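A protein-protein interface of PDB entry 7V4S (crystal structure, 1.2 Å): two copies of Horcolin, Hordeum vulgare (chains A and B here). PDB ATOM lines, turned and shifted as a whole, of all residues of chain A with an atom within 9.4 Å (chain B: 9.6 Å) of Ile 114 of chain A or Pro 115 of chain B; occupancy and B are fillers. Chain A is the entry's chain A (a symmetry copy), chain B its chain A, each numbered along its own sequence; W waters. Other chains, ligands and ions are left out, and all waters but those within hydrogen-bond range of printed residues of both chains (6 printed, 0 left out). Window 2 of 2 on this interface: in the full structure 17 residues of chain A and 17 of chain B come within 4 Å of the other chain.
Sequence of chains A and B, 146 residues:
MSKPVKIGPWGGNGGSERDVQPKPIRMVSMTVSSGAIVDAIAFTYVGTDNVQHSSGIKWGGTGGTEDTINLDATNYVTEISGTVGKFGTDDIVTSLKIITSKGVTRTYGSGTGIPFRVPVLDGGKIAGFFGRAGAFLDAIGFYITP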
ATOM      1  N   TRP A  10     -32.007  -2.708   9.741  1.00  0.00           N
ATOM      2  CA  TRP A  10     -30.601  -2.385  10.115  1.00  0.00           C
ATOM      3  C   TRP A  10     -29.685  -3.195   9.194  1.00  0.00           C
ATOM      4  O   TRP A  10     -29.828  -4.445   9.185  1.00  0.00           O
ATOM      5  CB  TRP A  10     -30.333  -2.693  11.594  1.00  0.00           C
ATOM      6  CG  TRP A  10     -31.128  -1.791  12.478  1.00  0.00           C
ATOM      7  CD1 TRP A  10     -30.772  -0.535  12.878  1.00  0.00           C
ATOM      8  CD2 TRP A  10     -32.477  -1.970  12.927  1.00  0.00           C
ATOM      9  NE1 TRP A  10     -31.792   0.036  13.619  1.00  0.00           N
ATOM     10  CE2 TRP A  10     -32.865  -0.805  13.621  1.00  0.00           C
ATOM     11  CE3 TRP A  10     -33.402  -2.990  12.819  1.00  0.00           C
ATOM     12  CZ2 TRP A  10     -34.087  -0.643  14.260  1.00  0.00           C
ATOM     13  CZ3 TRP A  10     -34.633  -2.816  13.412  1.00  0.00           C
ATOM     14  CH2 TRP A  10     -34.974  -1.665  14.100  1.00  0.00           C
ATOM     15  N   GLY A  11     -28.756  -2.535   8.527  1.00  0.00           N
ATOM     16  CA  GLY A  11     -27.820  -3.242   7.642  1.00  0.00           C
ATOM     17  C   GLY A  11     -27.514  -2.443   6.417  1.00  0.00           C
ATOM     18  O   GLY A  11     -27.738  -1.189   6.393  1.00  0.00           O
ATOM     19  N   SER A  81     -30.247  -7.883  19.236  1.00  0.00           N
ATOM     20  CA  SER A  81     -29.199  -6.900  18.950  1.00  0.00           C
ATOM     21  C   SER A  81     -28.233  -7.458  17.910  1.00  0.00           C
ATOM     22  O   SER A  81     -28.333  -8.671  17.573  1.00  0.00           O
ATOM     23  CB  SER A  81     -28.455  -6.527  20.209  1.00  0.00           C
ATOM     24  OG  SER A  81     -27.813  -7.654  20.759  1.00  0.00           O
ATOM     25  N   GLY A  82     -27.325  -6.635  17.449  1.00  0.00           N
ATOM     26  CA  GLY A  82     -26.396  -7.133  16.451  1.00  0.00           C
ATOM     27  C   GLY A  82     -25.443  -6.062  16.033  1.00  0.00           C
ATOM     28  O   GLY A  82     -25.370  -4.987  16.668  1.00  0.00           O
ATOM     29  N   THR A  83     -24.707  -6.304  14.946  1.00  0.00           N
ATOM     30  CA  THR A  83     -23.771  -5.338  14.387  1.00  0.00           C
ATOM     31  C   THR A  83     -23.842  -5.323  12.870  1.00  0.00           C
ATOM     32  O   THR A  83     -24.238  -6.365  12.274  1.00  0.00           O
ATOM     33  CB  THR A  83     -22.331  -5.668  14.792  1.00  0.00           C
ATOM     34  OG1 THR A  83     -22.024  -7.048  14.516  1.00  0.00           O
ATOM     35  CG2 THR A  83     -22.106  -5.444  16.271  1.00  0.00           C
ATOM     36  N   VAL A  84     -23.644  -4.175  12.303  1.00  0.00           N
ATOM     37  CA  VAL A  84     -23.601  -3.975  10.851  1.00  0.00           C
ATOM     38  C   VAL A  84     -22.201  -3.564  10.458  1.00  0.00           C
ATOM     39  O   VAL A  84     -21.636  -2.540  10.948  1.00  0.00           O
ATOM     40  CB  VAL A  84     -24.630  -2.930  10.390  1.00  0.00           C
ATOM     41  CG1 VAL A  84     -24.438  -2.600   8.922  1.00  0.00           C
ATOM     42  CG2 VAL A  84     -26.051  -3.366  10.724  1.00  0.00           C
ATOM     43  N   GLY A  85     -21.553  -4.365   9.636  1.00  0.00           N
ATOM     44  CA  GLY A  85     -20.162  -4.098   9.302  1.00  0.00           C
ATOM     45  C   GLY A  85     -19.772  -4.774   8.024  1.00  0.00           C
ATOM     46  O   GLY A  85     -20.632  -5.456   7.404  1.00  0.00           O
ATOM     47  N   LYS A  86     -18.508  -4.634   7.615  1.00  0.00           N
ATOM     48  CA  LYS A  86     -18.027  -5.244   6.368  1.00  0.00           C
ATOM     49  C   LYS A  86     -17.817  -6.740   6.567  1.00  0.00           C
ATOM     50  O   LYS A  86     -17.363  -7.223   7.629  1.00  0.00           O
ATOM     51  CB  LYS A  86     -16.685  -4.649   5.939  1.00  0.00           C
ATOM     52  CG  LYS A  86     -16.784  -3.218   5.503  1.00  0.00           C
ATOM     53  CD  LYS A  86     -17.560  -3.067   4.242  1.00  0.00           C
ATOM     54  CE  LYS A  86     -17.320  -1.725   3.580  1.00  0.00           C
ATOM     55  NZ  LYS A  86     -18.260  -1.536   2.459  1.00  0.00           N
ATOM     56  N   ASP A  91     -21.552  -4.074   3.395  1.00  0.00           N
ATOM     57  CA  ASP A  91     -22.066  -3.891   4.763  1.00  0.00           C
ATOM     58  C   ASP A  91     -23.226  -4.864   4.988  1.00  0.00           C
ATOM     59  O   ASP A  91     -24.254  -4.779   4.266  1.00  0.00           O
ATOM     60  CB  ASP A  91     -22.546  -2.446   4.956  1.00  0.00           C
ATOM     61  CG  ASP A  91     -21.447  -1.437   5.277  1.00  0.00           C
ATOM     62  OD1 ASP A  91     -20.381  -1.865   5.758  1.00  0.00           O
ATOM     63  OD2 ASP A  91     -21.706  -0.218   5.105  1.00  0.00           O
ATOM     64  N   ILE A  92     -23.097  -5.714   5.976  1.00  0.00           N
ATOM     65  CA  ILE A  92     -24.133  -6.748   6.227  1.00  0.00           C
ATOM     66  C   ILE A  92     -24.363  -6.846   7.714  1.00  0.00           C
ATOM     67  O   ILE A  92     -23.661  -6.189   8.541  1.00  0.00           O
ATOM     68  CB  ILE A  92     -23.696  -8.089   5.624  1.00  0.00           C
ATOM     69  CG1 ILE A  92     -22.448  -8.672   6.312  1.00  0.00           C
ATOM     70  CG2 ILE A  92     -23.484  -8.009   4.128  1.00  0.00           C
ATOM     71  CD1 ILE A  92     -22.277 -10.135   6.069  1.00  0.00           C
ATOM     72  N   VAL A  93     -25.211  -7.772   8.096  1.00  0.00           N
ATOM     73  CA  VAL A  93     -25.390  -8.092   9.522  1.00  0.00           C
ATOM     74  C   VAL A  93     -24.269  -9.066   9.864  1.00  0.00           C
ATOM     75  O   VAL A  93     -24.280 -10.279   9.512  1.00  0.00           O
ATOM     76  CB  VAL A  93     -26.755  -8.725   9.742  1.00  0.00           C
ATOM     77  CG1 VAL A  93     -26.946  -9.119  11.165  1.00  0.00           C
ATOM     78  CG2 VAL A  93     -27.849  -7.731   9.352  1.00  0.00           C
ATOM     79  N   THR A  94     -23.311  -8.574  10.633  1.00  0.00           N
ATOM     80  CA  THR A  94     -22.093  -9.371  10.949  1.00  0.00           C
ATOM     81  C   THR A  94     -22.270 -10.139  12.241  1.00  0.00           C
ATOM     82  O   THR A  94     -21.485 -11.126  12.450  1.00  0.00           O
ATOM     83  CB  THR A  94     -20.866  -8.466  11.018  1.00  0.00           C
ATOM     84  OG1 THR A  94     -21.167  -7.398  11.915  1.00  0.00           O
ATOM     85  CG2 THR A  94     -20.505  -7.914   9.673  1.00  0.00           C
ATOM     86  N   SER A  95     -23.220  -9.801  13.089  1.00  0.00           N
ATOM     87  CA  SER A  95     -23.561 -10.610  14.275  1.00  0.00           C
ATOM     88  C   SER A  95     -25.027 -10.339  14.619  1.00  0.00           C
ATOM     89  O   SER A  95     -25.518  -9.252  14.329  1.00  0.00           O
ATOM     90  CB  SER A  95     -22.651 -10.331  15.467  1.00  0.00           C
ATOM     91  OG  SER A  95     -22.875  -9.007  15.992  1.00  0.00           O
ATOM     92  N   GLY A 111     -18.730 -11.334  13.958  1.00  0.00           N
ATOM     93  CA  GLY A 111     -18.291 -10.073  13.362  1.00  0.00           C
ATOM     94  C   GLY A 111     -18.539  -8.877  14.251  1.00  0.00           C
ATOM     95  O   GLY A 111     -19.041  -9.029  15.383  1.00  0.00           O
ATOM     96  N   THR A 112     -18.124  -7.740  13.700  1.00  0.00           N
ATOM     97  CA  THR A 112     -18.135  -6.426  14.370  1.00  0.00           C
ATOM     98  C   THR A 112     -18.720  -5.356  13.443  1.00  0.00           C
ATOM     99  O   THR A 112     -19.012  -5.679  12.307  1.00  0.00           O
ATOM    100  CB  THR A 112     -16.674  -6.059  14.680  1.00  0.00           C
ATOM    101  OG1 THR A 112     -15.975  -5.989  13.432  1.00  0.00           O
ATOM    102  CG2 THR A 112     -15.980  -7.020  15.632  1.00  0.00           C
ATOM    103  N   GLY A 113     -18.684  -4.113  13.897  1.00  0.00           N
ATOM    104  CA  GLY A 113     -19.194  -2.933  13.185  1.00  0.00           C
ATOM    105  C   GLY A 113     -20.105  -2.122  14.100  1.00  0.00           C
ATOM    106  O   GLY A 113     -19.981  -2.061  15.329  1.00  0.00           O
ATOM    107  N   ILE A 114     -21.056  -1.416  13.489  1.00  0.00           N
ATOM    108  CA  ILE A 114     -21.945  -0.465  14.222  1.00  0.00           C
ATOM    109  C   ILE A 114     -23.039  -1.262  14.949  1.00  0.00           C
ATOM    110  O   ILE A 114     -23.730  -2.047  14.320  1.00  0.00           O
ATOM    111  CB  ILE A 114     -22.520   0.558  13.223  1.00  0.00           C
ATOM    112  CG1 ILE A 114     -21.407   1.317  12.496  1.00  0.00           C
ATOM    113  CG2 ILE A 114     -23.474   1.501  13.957  1.00  0.00           C
ATOM    114  CD1 ILE A 114     -21.907   2.400  11.572  1.00  0.00           C
ATOM    115  N   PRO A 115     -23.191  -1.144  16.270  1.00  0.00           N
ATOM    116  CA  PRO A 115     -24.200  -1.919  16.964  1.00  0.00           C
ATOM    117  C   PRO A 115     -25.619  -1.357  16.805  1.00  0.00           C
ATOM    118  O   PRO A 115     -25.802  -0.184  16.619  1.00  0.00           O
ATOM    119  CB  PRO A 115     -23.725  -1.816  18.419  1.00  0.00           C
ATOM    120  CG  PRO A 115     -23.192  -0.402  18.449  1.00  0.00           C
ATOM    121  CD  PRO A 115     -22.391  -0.301  17.169  1.00  0.00           C
ATOM    122  N   PHE A 116     -26.548  -2.293  16.753  1.00  0.00           N
ATOM    123  CA  PHE A 116     -27.989  -1.952  16.879  1.00  0.00           C
ATOM    124  C   PHE A 116     -28.568  -2.849  17.985  1.00  0.00           C
ATOM    125  O   PHE A 116     -28.088  -3.947  18.215  1.00  0.00           O
ATOM    126  CB  PHE A 116     -28.742  -2.094  15.551  1.00  0.00           C
ATOM    127  CG  PHE A 116     -28.838  -3.516  15.024  1.00  0.00           C
ATOM    128  CD1 PHE A 116     -29.890  -4.361  15.359  1.00  0.00           C
ATOM    129  CD2 PHE A 116     -27.852  -3.993  14.167  1.00  0.00           C
ATOM    130  CE1 PHE A 116     -29.953  -5.649  14.843  1.00  0.00           C
ATOM    131  CE2 PHE A 116     -27.911  -5.291  13.680  1.00  0.00           C
ATOM    132  CZ  PHE A 116     -28.973  -6.103  13.990  1.00  0.00           C
ATOM    133  N   ARG A 117     -29.593  -2.358  18.659  1.00  0.00           N
ATOM    134  CA  ARG A 117     -30.238  -3.100  19.759  1.00  0.00           C
ATOM    135  C   ARG A 117     -31.698  -2.688  19.863  1.00  0.00           C
ATOM    136  O   ARG A 117     -31.986  -1.515  19.886  1.00  0.00           O
ATOM    137  CB  ARG A 117     -29.474  -2.818  21.052  1.00  0.00           C
ATOM    138  CG  ARG A 117     -30.096  -3.458  22.280  1.00  0.00           C
ATOM    139  CD  ARG A 117     -29.198  -3.322  23.509  1.00  0.00           C
ATOM    140  NE  ARG A 117     -29.790  -3.975  24.654  1.00  0.00           N
ATOM    141  CZ  ARG A 117     -30.246  -3.413  25.758  1.00  0.00           C
ATOM    142  NH1 ARG A 117     -30.808  -4.169  26.680  1.00  0.00           N
ATOM    143  NH2 ARG A 117     -30.244  -2.117  25.910  1.00  0.00           N
ATOM    144  N   TRP B  10     -32.158   3.936  24.372  1.00  0.00           N
ATOM    145  CA  TRP B  10     -30.809   4.156  23.779  1.00  0.00           C
ATOM    146  C   TRP B  10     -30.139   5.280  24.574  1.00  0.00           C
ATOM    147  O   TRP B  10     -30.740   6.383  24.642  1.00  0.00           O
ATOM    148  CB  TRP B  10     -30.905   4.499  22.286  1.00  0.00           C
ATOM    149  CG  TRP B  10     -31.425   3.337  21.506  1.00  0.00           C
ATOM    150  CD1 TRP B  10     -30.686   2.298  21.019  1.00  0.00           C
ATOM    151  CD2 TRP B  10     -32.793   2.981  21.273  1.00  0.00           C
ATOM    152  NE1 TRP B  10     -31.514   1.362  20.425  1.00  0.00           N
ATOM    153  CE2 TRP B  10     -32.812   1.734  20.611  1.00  0.00           C
ATOM    154  CE3 TRP B  10     -34.007   3.578  21.551  1.00  0.00           C
ATOM    155  CZ2 TRP B  10     -33.964   1.104  20.161  1.00  0.00           C
ATOM    156  CZ3 TRP B  10     -35.155   2.935  21.145  1.00  0.00           C
ATOM    157  CH2 TRP B  10     -35.136   1.720  20.484  1.00  0.00           C
ATOM    158  N   GLY B  11     -28.940   5.040  25.072  1.00  0.00           N
ATOM    159  CA  GLY B  11     -28.217   6.074  25.827  1.00  0.00           C
ATOM    160  C   GLY B  11     -27.450   5.487  26.966  1.00  0.00           C
ATOM    161  O   GLY B  11     -27.178   4.243  26.986  1.00  0.00           O
ATOM    162  N   ILE B  80     -37.182   8.196  14.204  1.00  0.00           N
ATOM    163  CA  ILE B  80     -36.285   8.962  15.091  1.00  0.00           C
ATOM    164  C   ILE B  80     -34.943   8.287  14.996  1.00  0.00           C
ATOM    165  O   ILE B  80     -34.849   7.037  15.089  1.00  0.00           O
ATOM    166  CB  ILE B  80     -36.810   9.051  16.523  1.00  0.00           C
ATOM    167  CG1 ILE B  80     -38.166   9.746  16.532  1.00  0.00           C
ATOM    168  CG2 ILE B  80     -35.797   9.703  17.446  1.00  0.00           C
ATOM    169  CD1 ILE B  80     -38.749   9.966  17.916  1.00  0.00           C
ATOM    170  N   SER B  81     -33.945   9.106  14.878  1.00  0.00           N
ATOM    171  CA  SER B  81     -32.573   8.600  14.972  1.00  0.00           C
ATOM    172  C   SER B  81     -31.744   9.513  15.870  1.00  0.00           C
ATOM    173  O   SER B  81     -32.243  10.608  16.255  1.00  0.00           O
ATOM    174  CB  SER B  81     -31.944   8.498  13.605  1.00  0.00           C
ATOM    175  OG  SER B  81     -31.867   9.767  12.998  1.00  0.00           O
ATOM    176  N   GLY B  82     -30.534   9.107  16.163  1.00  0.00           N
ATOM    177  CA  GLY B  82     -29.723   9.949  17.024  1.00  0.00           C
ATOM    178  C   GLY B  82     -28.385   9.330  17.259  1.00  0.00           C
ATOM    179  O   GLY B  82     -28.007   8.344  16.589  1.00  0.00           O
ATOM    180  N   THR B  83     -27.638   9.866  18.229  1.00  0.00           N
ATOM    181  CA  THR B  83     -26.333   9.342  18.611  1.00  0.00           C
ATOM    182  C   THR B  83     -26.163   9.346  20.119  1.00  0.00           C
ATOM    183  O   THR B  83     -26.828  10.179  20.800  1.00  0.00           O
ATOM    184  CB  THR B  83     -25.204  10.178  18.002  1.00  0.00           C
ATOM    185  OG1 THR B  83     -25.403  11.580  18.270  1.00  0.00           O
ATOM    186  CG2 THR B  83     -25.139  10.011  16.500  1.00  0.00           C
ATOM    187  N   VAL B  84     -25.462   8.376  20.616  1.00  0.00           N
ATOM    188  CA  VAL B  84     -25.127   8.250  22.038  1.00  0.00           C
ATOM    189  C   VAL B  84     -23.634   8.410  22.201  1.00  0.00           C
ATOM    190  O   VAL B  84     -22.806   7.661  21.600  1.00  0.00           O
ATOM    191  CB  VAL B  84     -25.603   6.908  22.617  1.00  0.00           C
ATOM    192  CG1 VAL B  84     -25.080   6.719  24.029  1.00  0.00           C
ATOM    193  CG2 VAL B  84     -27.115   6.765  22.517  1.00  0.00           C
ATOM    194  N   GLY B  85     -23.219   9.421  22.939  1.00  0.00           N
ATOM    195  CA  GLY B  85     -21.797   9.709  23.049  1.00  0.00           C
ATOM    196  C   GLY B  85     -21.501  10.520  24.274  1.00  0.00           C
ATOM    197  O   GLY B  85     -22.451  10.845  25.037  1.00  0.00           O
ATOM    198  N   ILE B  92     -24.584  10.196  26.829  1.00  0.00           N
ATOM    199  CA  ILE B  92     -25.959  10.754  26.770  1.00  0.00           C
ATOM    200  C   ILE B  92     -26.431  10.713  25.339  1.00  0.00           C
ATOM    201  O   ILE B  92     -25.668  10.346  24.395  1.00  0.00           O
ATOM    202  CB  ILE B  92     -25.975  12.178  27.339  1.00  0.00           C
ATOM    203  CG1 ILE B  92     -25.159  13.168  26.488  1.00  0.00           C
ATOM    204  CG2 ILE B  92     -25.524  12.229  28.782  1.00  0.00           C
ATOM    205  CD1 ILE B  92     -25.518  14.594  26.746  1.00  0.00           C
ATOM    206  N   THR B  94     -26.566  12.623  22.347  1.00  0.00           N
ATOM    207  CA  THR B  94     -25.802  13.811  21.873  1.00  0.00           C
ATOM    208  C   THR B  94     -26.450  14.415  20.647  1.00  0.00           C
ATOM    209  O   THR B  94     -26.138  15.619  20.351  1.00  0.00           O
ATOM    210  CB  THR B  94     -24.350  13.434  21.592  1.00  0.00           C
ATOM    211  OG1 THR B  94     -24.359  12.305  20.719  1.00  0.00           O
ATOM    212  CG2 THR B  94     -23.608  13.100  22.849  1.00  0.00           C
ATOM    213  N   SER B  95     -27.318  13.718  19.943  1.00  0.00           N
ATOM    214  CA  SER B  95     -28.115  14.303  18.847  1.00  0.00           C
ATOM    215  C   SER B  95     -29.405  13.488  18.722  1.00  0.00           C
ATOM    216  O   SER B  95     -29.398  12.306  19.050  1.00  0.00           O
ATOM    217  CB  SER B  95     -27.360  14.353  17.523  1.00  0.00           C
ATOM    218  OG  SER B  95     -27.144  13.028  16.999  1.00  0.00           O
ATOM    219  N   LYS B  97     -32.716  13.246  15.635  1.00  0.00           N
ATOM    220  CA  LYS B  97     -33.356  13.665  14.394  1.00  0.00           C
ATOM    221  C   LYS B  97     -34.760  13.090  14.384  1.00  0.00           C
ATOM    222  O   LYS B  97     -34.932  11.873  14.638  1.00  0.00           O
ATOM    223  CB  LYS B  97     -32.497  13.205  13.222  1.00  0.00           C
ATOM    224  CG  LYS B  97     -33.052  13.484  11.849  1.00  0.00           C
ATOM    225  CD  LYS B  97     -32.081  13.081  10.734  1.00  0.00           C
ATOM    226  CE  LYS B  97     -30.893  14.015  10.611  1.00  0.00           C
ATOM    227  NZ  LYS B  97     -29.763  13.620  11.481  1.00  0.00           N
ATOM    228  N   GLY B 111     -23.928  16.806  18.449  1.00  0.00           N
ATOM    229  CA  GLY B 111     -22.961  15.823  18.934  1.00  0.00           C
ATOM    230  C   GLY B 111     -22.870  14.596  18.057  1.00  0.00           C
ATOM    231  O   GLY B 111     -23.558  14.514  17.019  1.00  0.00           O
ATOM    232  N   THR B 112     -21.979  13.717  18.505  1.00  0.00           N
ATOM    233  CA  THR B 112     -21.593  12.478  17.805  1.00  0.00           C
ATOM    234  C   THR B 112     -21.583  11.294  18.777  1.00  0.00           C
ATOM    235  O   THR B 112     -21.800  11.516  19.954  1.00  0.00           O
ATOM    236  CB  THR B 112     -20.168  12.680  17.266  1.00  0.00           C
ATOM    237  OG1 THR B 112     -19.314  12.917  18.391  1.00  0.00           O
ATOM    238  CG2 THR B 112     -20.041  13.803  16.249  1.00  0.00           C
ATOM    239  N   GLY B 113     -21.150  10.143  18.286  1.00  0.00           N
ATOM    240  CA  GLY B 113     -21.063   8.881  19.031  1.00  0.00           C
ATOM    241  C   GLY B 113     -21.727   7.758  18.242  1.00  0.00           C
ATOM    242  O   GLY B 113     -21.777   7.711  17.007  1.00  0.00           O
ATOM    243  N   ILE B 114     -22.236   6.763  18.968  1.00  0.00           N
ATOM    244  CA  ILE B 114     -22.800   5.527  18.350  1.00  0.00           C
ATOM    245  C   ILE B 114     -24.211   5.828  17.822  1.00  0.00           C
ATOM    246  O   ILE B 114     -25.043   6.313  18.572  1.00  0.00           O
ATOM    247  CB  ILE B 114     -22.788   4.392  19.394  1.00  0.00           C
ATOM    248  CG1 ILE B 114     -21.374   4.132  19.921  1.00  0.00           C
ATOM    249  CG2 ILE B 114     -23.414   3.137  18.786  1.00  0.00           C
ATOM    250  CD1 ILE B 114     -21.281   2.968  20.877  1.00  0.00           C
ATOM    251  N   PRO B 115     -24.505   5.622  16.537  1.00  0.00           N
ATOM    252  CA  PRO B 115     -25.825   5.939  16.027  1.00  0.00           C
ATOM    253  C   PRO B 115     -26.884   4.887  16.383  1.00  0.00           C
ATOM    254  O   PRO B 115     -26.581   3.737  16.559  1.00  0.00           O
ATOM    255  CB  PRO B 115     -25.573   5.978  14.515  1.00  0.00           C
ATOM    256  CG  PRO B 115     -24.557   4.871  14.361  1.00  0.00           C
ATOM    257  CD  PRO B 115     -23.592   5.118  15.502  1.00  0.00           C
ATOM    258  N   PHE B 116     -28.079   5.404  16.603  1.00  0.00           N
ATOM    259  CA  PHE B 116     -29.285   4.540  16.687  1.00  0.00           C
ATOM    260  C   PHE B 116     -30.322   5.119  15.708  1.00  0.00           C
ATOM    261  O   PHE B 116     -30.332   6.309  15.442  1.00  0.00           O
ATOM    262  CB  PHE B 116     -29.826   4.427  18.117  1.00  0.00           C
ATOM    263  CG  PHE B 116     -30.370   5.722  18.695  1.00  0.00           C
ATOM    264  CD1 PHE B 116     -31.701   6.097  18.549  1.00  0.00           C
ATOM    265  CD2 PHE B 116     -29.519   6.562  19.407  1.00  0.00           C
ATOM    266  CE1 PHE B 116     -32.166   7.281  19.107  1.00  0.00           C
ATOM    267  CE2 PHE B 116     -29.990   7.756  19.936  1.00  0.00           C
ATOM    268  CZ  PHE B 116     -31.313   8.097  19.814  1.00  0.00           C
ATOM    269  N   ARG B 117     -31.174   4.257  15.184  1.00  0.00           N
ATOM    270  CA  ARG B 117     -32.211   4.667  14.217  1.00  0.00           C
ATOM    271  C   ARG B 117     -33.404   3.731  14.324  1.00  0.00           C
ATOM    272  O   ARG B 117     -33.227   2.536  14.309  1.00  0.00           O
ATOM    273  CB  ARG B 117     -31.602   4.656  12.815  1.00  0.00           C
ATOM    274  CG  ARG B 117     -32.598   4.976  11.716  1.00  0.00           C
ATOM    275  CD  ARG B 117     -31.913   5.153  10.361  1.00  0.00           C
ATOM    276  NE  ARG B 117     -32.874   5.499   9.340  1.00  0.00           N
ATOM    277  CZ  ARG B 117     -33.246   4.774   8.301  1.00  0.00           C
ATOM    278  NH1 ARG B 117     -34.184   5.234   7.498  1.00  0.00           N
ATOM    279  NH2 ARG B 117     -32.778   3.571   8.112  1.00  0.00           N
ATOM    280  N   VAL B 118     -34.562   4.332  14.461  1.00  0.00           N
ATOM    281  CA  VAL B 118     -35.817   3.538  14.482  1.00  0.00           C
ATOM    282  C   VAL B 118     -36.760   4.063  13.403  1.00  0.00           C
ATOM    283  O   VAL B 118     -37.520   5.024  13.630  1.00  0.00           O
ATOM    284  CB  VAL B 118     -36.487   3.526  15.863  1.00  0.00           C
ATOM    285  CG1 VAL B 118     -37.772   2.732  15.795  1.00  0.00           C
ATOM    286  CG2 VAL B 118     -35.539   2.927  16.912  1.00  0.00           C
HETATM  287  O   HOH W   1     -29.710   0.563  18.180  1.00  0.00           O
HETATM  288  O   HOH W   2     -30.106   1.524  15.587  1.00  0.00           O
HETATM  289  O   HOH W   3     -27.199   1.559  18.633  1.00  0.00           O
HETATM  290  O   HOH W   4     -32.416   1.458  11.230  1.00  0.00           O
HETATM  291  O   HOH W   5     -27.504   1.537  14.729  1.00  0.00           O
HETATM  292  O   HOH W   6     -31.184  -0.119  22.838  1.00  0.00           O
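The backbone carbonyl oxygen (O) of Arg 117 of chain B is in hydrogen-bond range of the indole nitrogen (NE1) of Trp 10 of chain A, at 3.0 Å.
O of Arg 117 of chain A is in hydrogen-bond range of NE1 of Trp 10 of chain B, 3.0 Å away.
O of Val 84 of chain B sits at hydrogen-bond distance from N of Ile 114 of chain B, at 2.8 Å.
The backbone carbonyl oxygen (O) of Val 84 of chain A is in hydrogen-bond range of the backbone NH (N) of Ile 114 of chain A (2.8 Å).
CG2 of Ile 114 of chain A touches CG of Pro 115 of chain B, at 3.6 Å.
CG2 of Ile 114 of chain B touches CG of Pro 115 of chain A (3.6 Å).
Pro 115 of chain A touches Pro 115 of chain B (O to O, 3.998 Å).
Ile 114 of chain A touches just one residue of chain B: Pro 115.
Of the printed residues of chain A, Pro 115 of chain B touches Ile 114 (3.6 Å) and Pro 115 (3.998 Å).
Thr 83 of chain A touches none of the printed residues of chain B.
No residue of chain B comes within 4 Å of Gly 113 of chain A.
Of the printed residues of chain A, Arg 117 of chain B touches Trp 10 (3.0 Å).
Of the printed residues of chain B, Trp 10 of chain A touches Arg 117.
Printed residues of chain A within 4 Å of Trp 10 of chain B: Arg 117.
Printed residues of chain B within 4 Å of Arg 117 of chain A: Trp 10 (3.0 Å).
Printed residues of chain A within 4 Å of Ile 114 of chain B: Pro 115 (3.6 Å).
Phe 116 of chain A touches none of the printed residues of chain B.
The nearest printed residue of chain B that does not touch Pro 115 of chain A is Phe 116 of chain B (5.9 Å).
Printed residues of chain A that touch a printed residue of chain B: Trp 10, Ile 114, Pro 115 and Arg 117.
Of the 20 printed residues of chain B, 4 touch a printed residue of chain A.
Among the printed residues, no Asp or Glu carboxylate lies within 4 Å of a Lys or Arg side-chain nitrogen of the other chain.
Trp 10 of chain A touches Arg 117 of chain B, and with the chains exchanged Arg 117 of chain A touches Trp 10 of chain B.
Ile 114 of chain A touches Pro 115 of chain B, and with the chains exchanged Pro 115 of chain A touches Ile 114 of chain B.
Pro 115 of chain B touches its own counterpart, Pro 115 of chain A.
Of the 5 pairs that touch across the chains among the printed residues, 5 have their exchanged pair printed and touching as well.
Water W4 lies within hydrogen-bond range of the indole nitrogen of Trp 10 of chain A (2.8 Å) and the backbone carbonyl oxygen of Arg 117 of chain B (3.4 Å).
Water W6 lies within hydrogen-bond range of the indole nitrogen of Trp 10 of chain B (2.9 Å) and the backbone carbonyl oxygen of Arg 117 of chain A (3.4 Å).
Water W2 bridges the backbone NH (N) of Arg 117 of chain B and the indole nitrogen (NE1) of Trp 10 of chain A.
Water W1 bridges the backbone NH of Arg 117 of chain A (3.0 Å) and the indole nitrogen of Trp 10 of chain B (3.0 Å).
Water W5 bridges O of Pro 115 of chain B (3.0 Å) and O of Pro 115 of chain A (3.1 Å).
Water W3 lies within hydrogen-bond range of O of Pro 115 of chain A (3.0 Å) and O of Pro 115 of chain B (3.1 Å).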
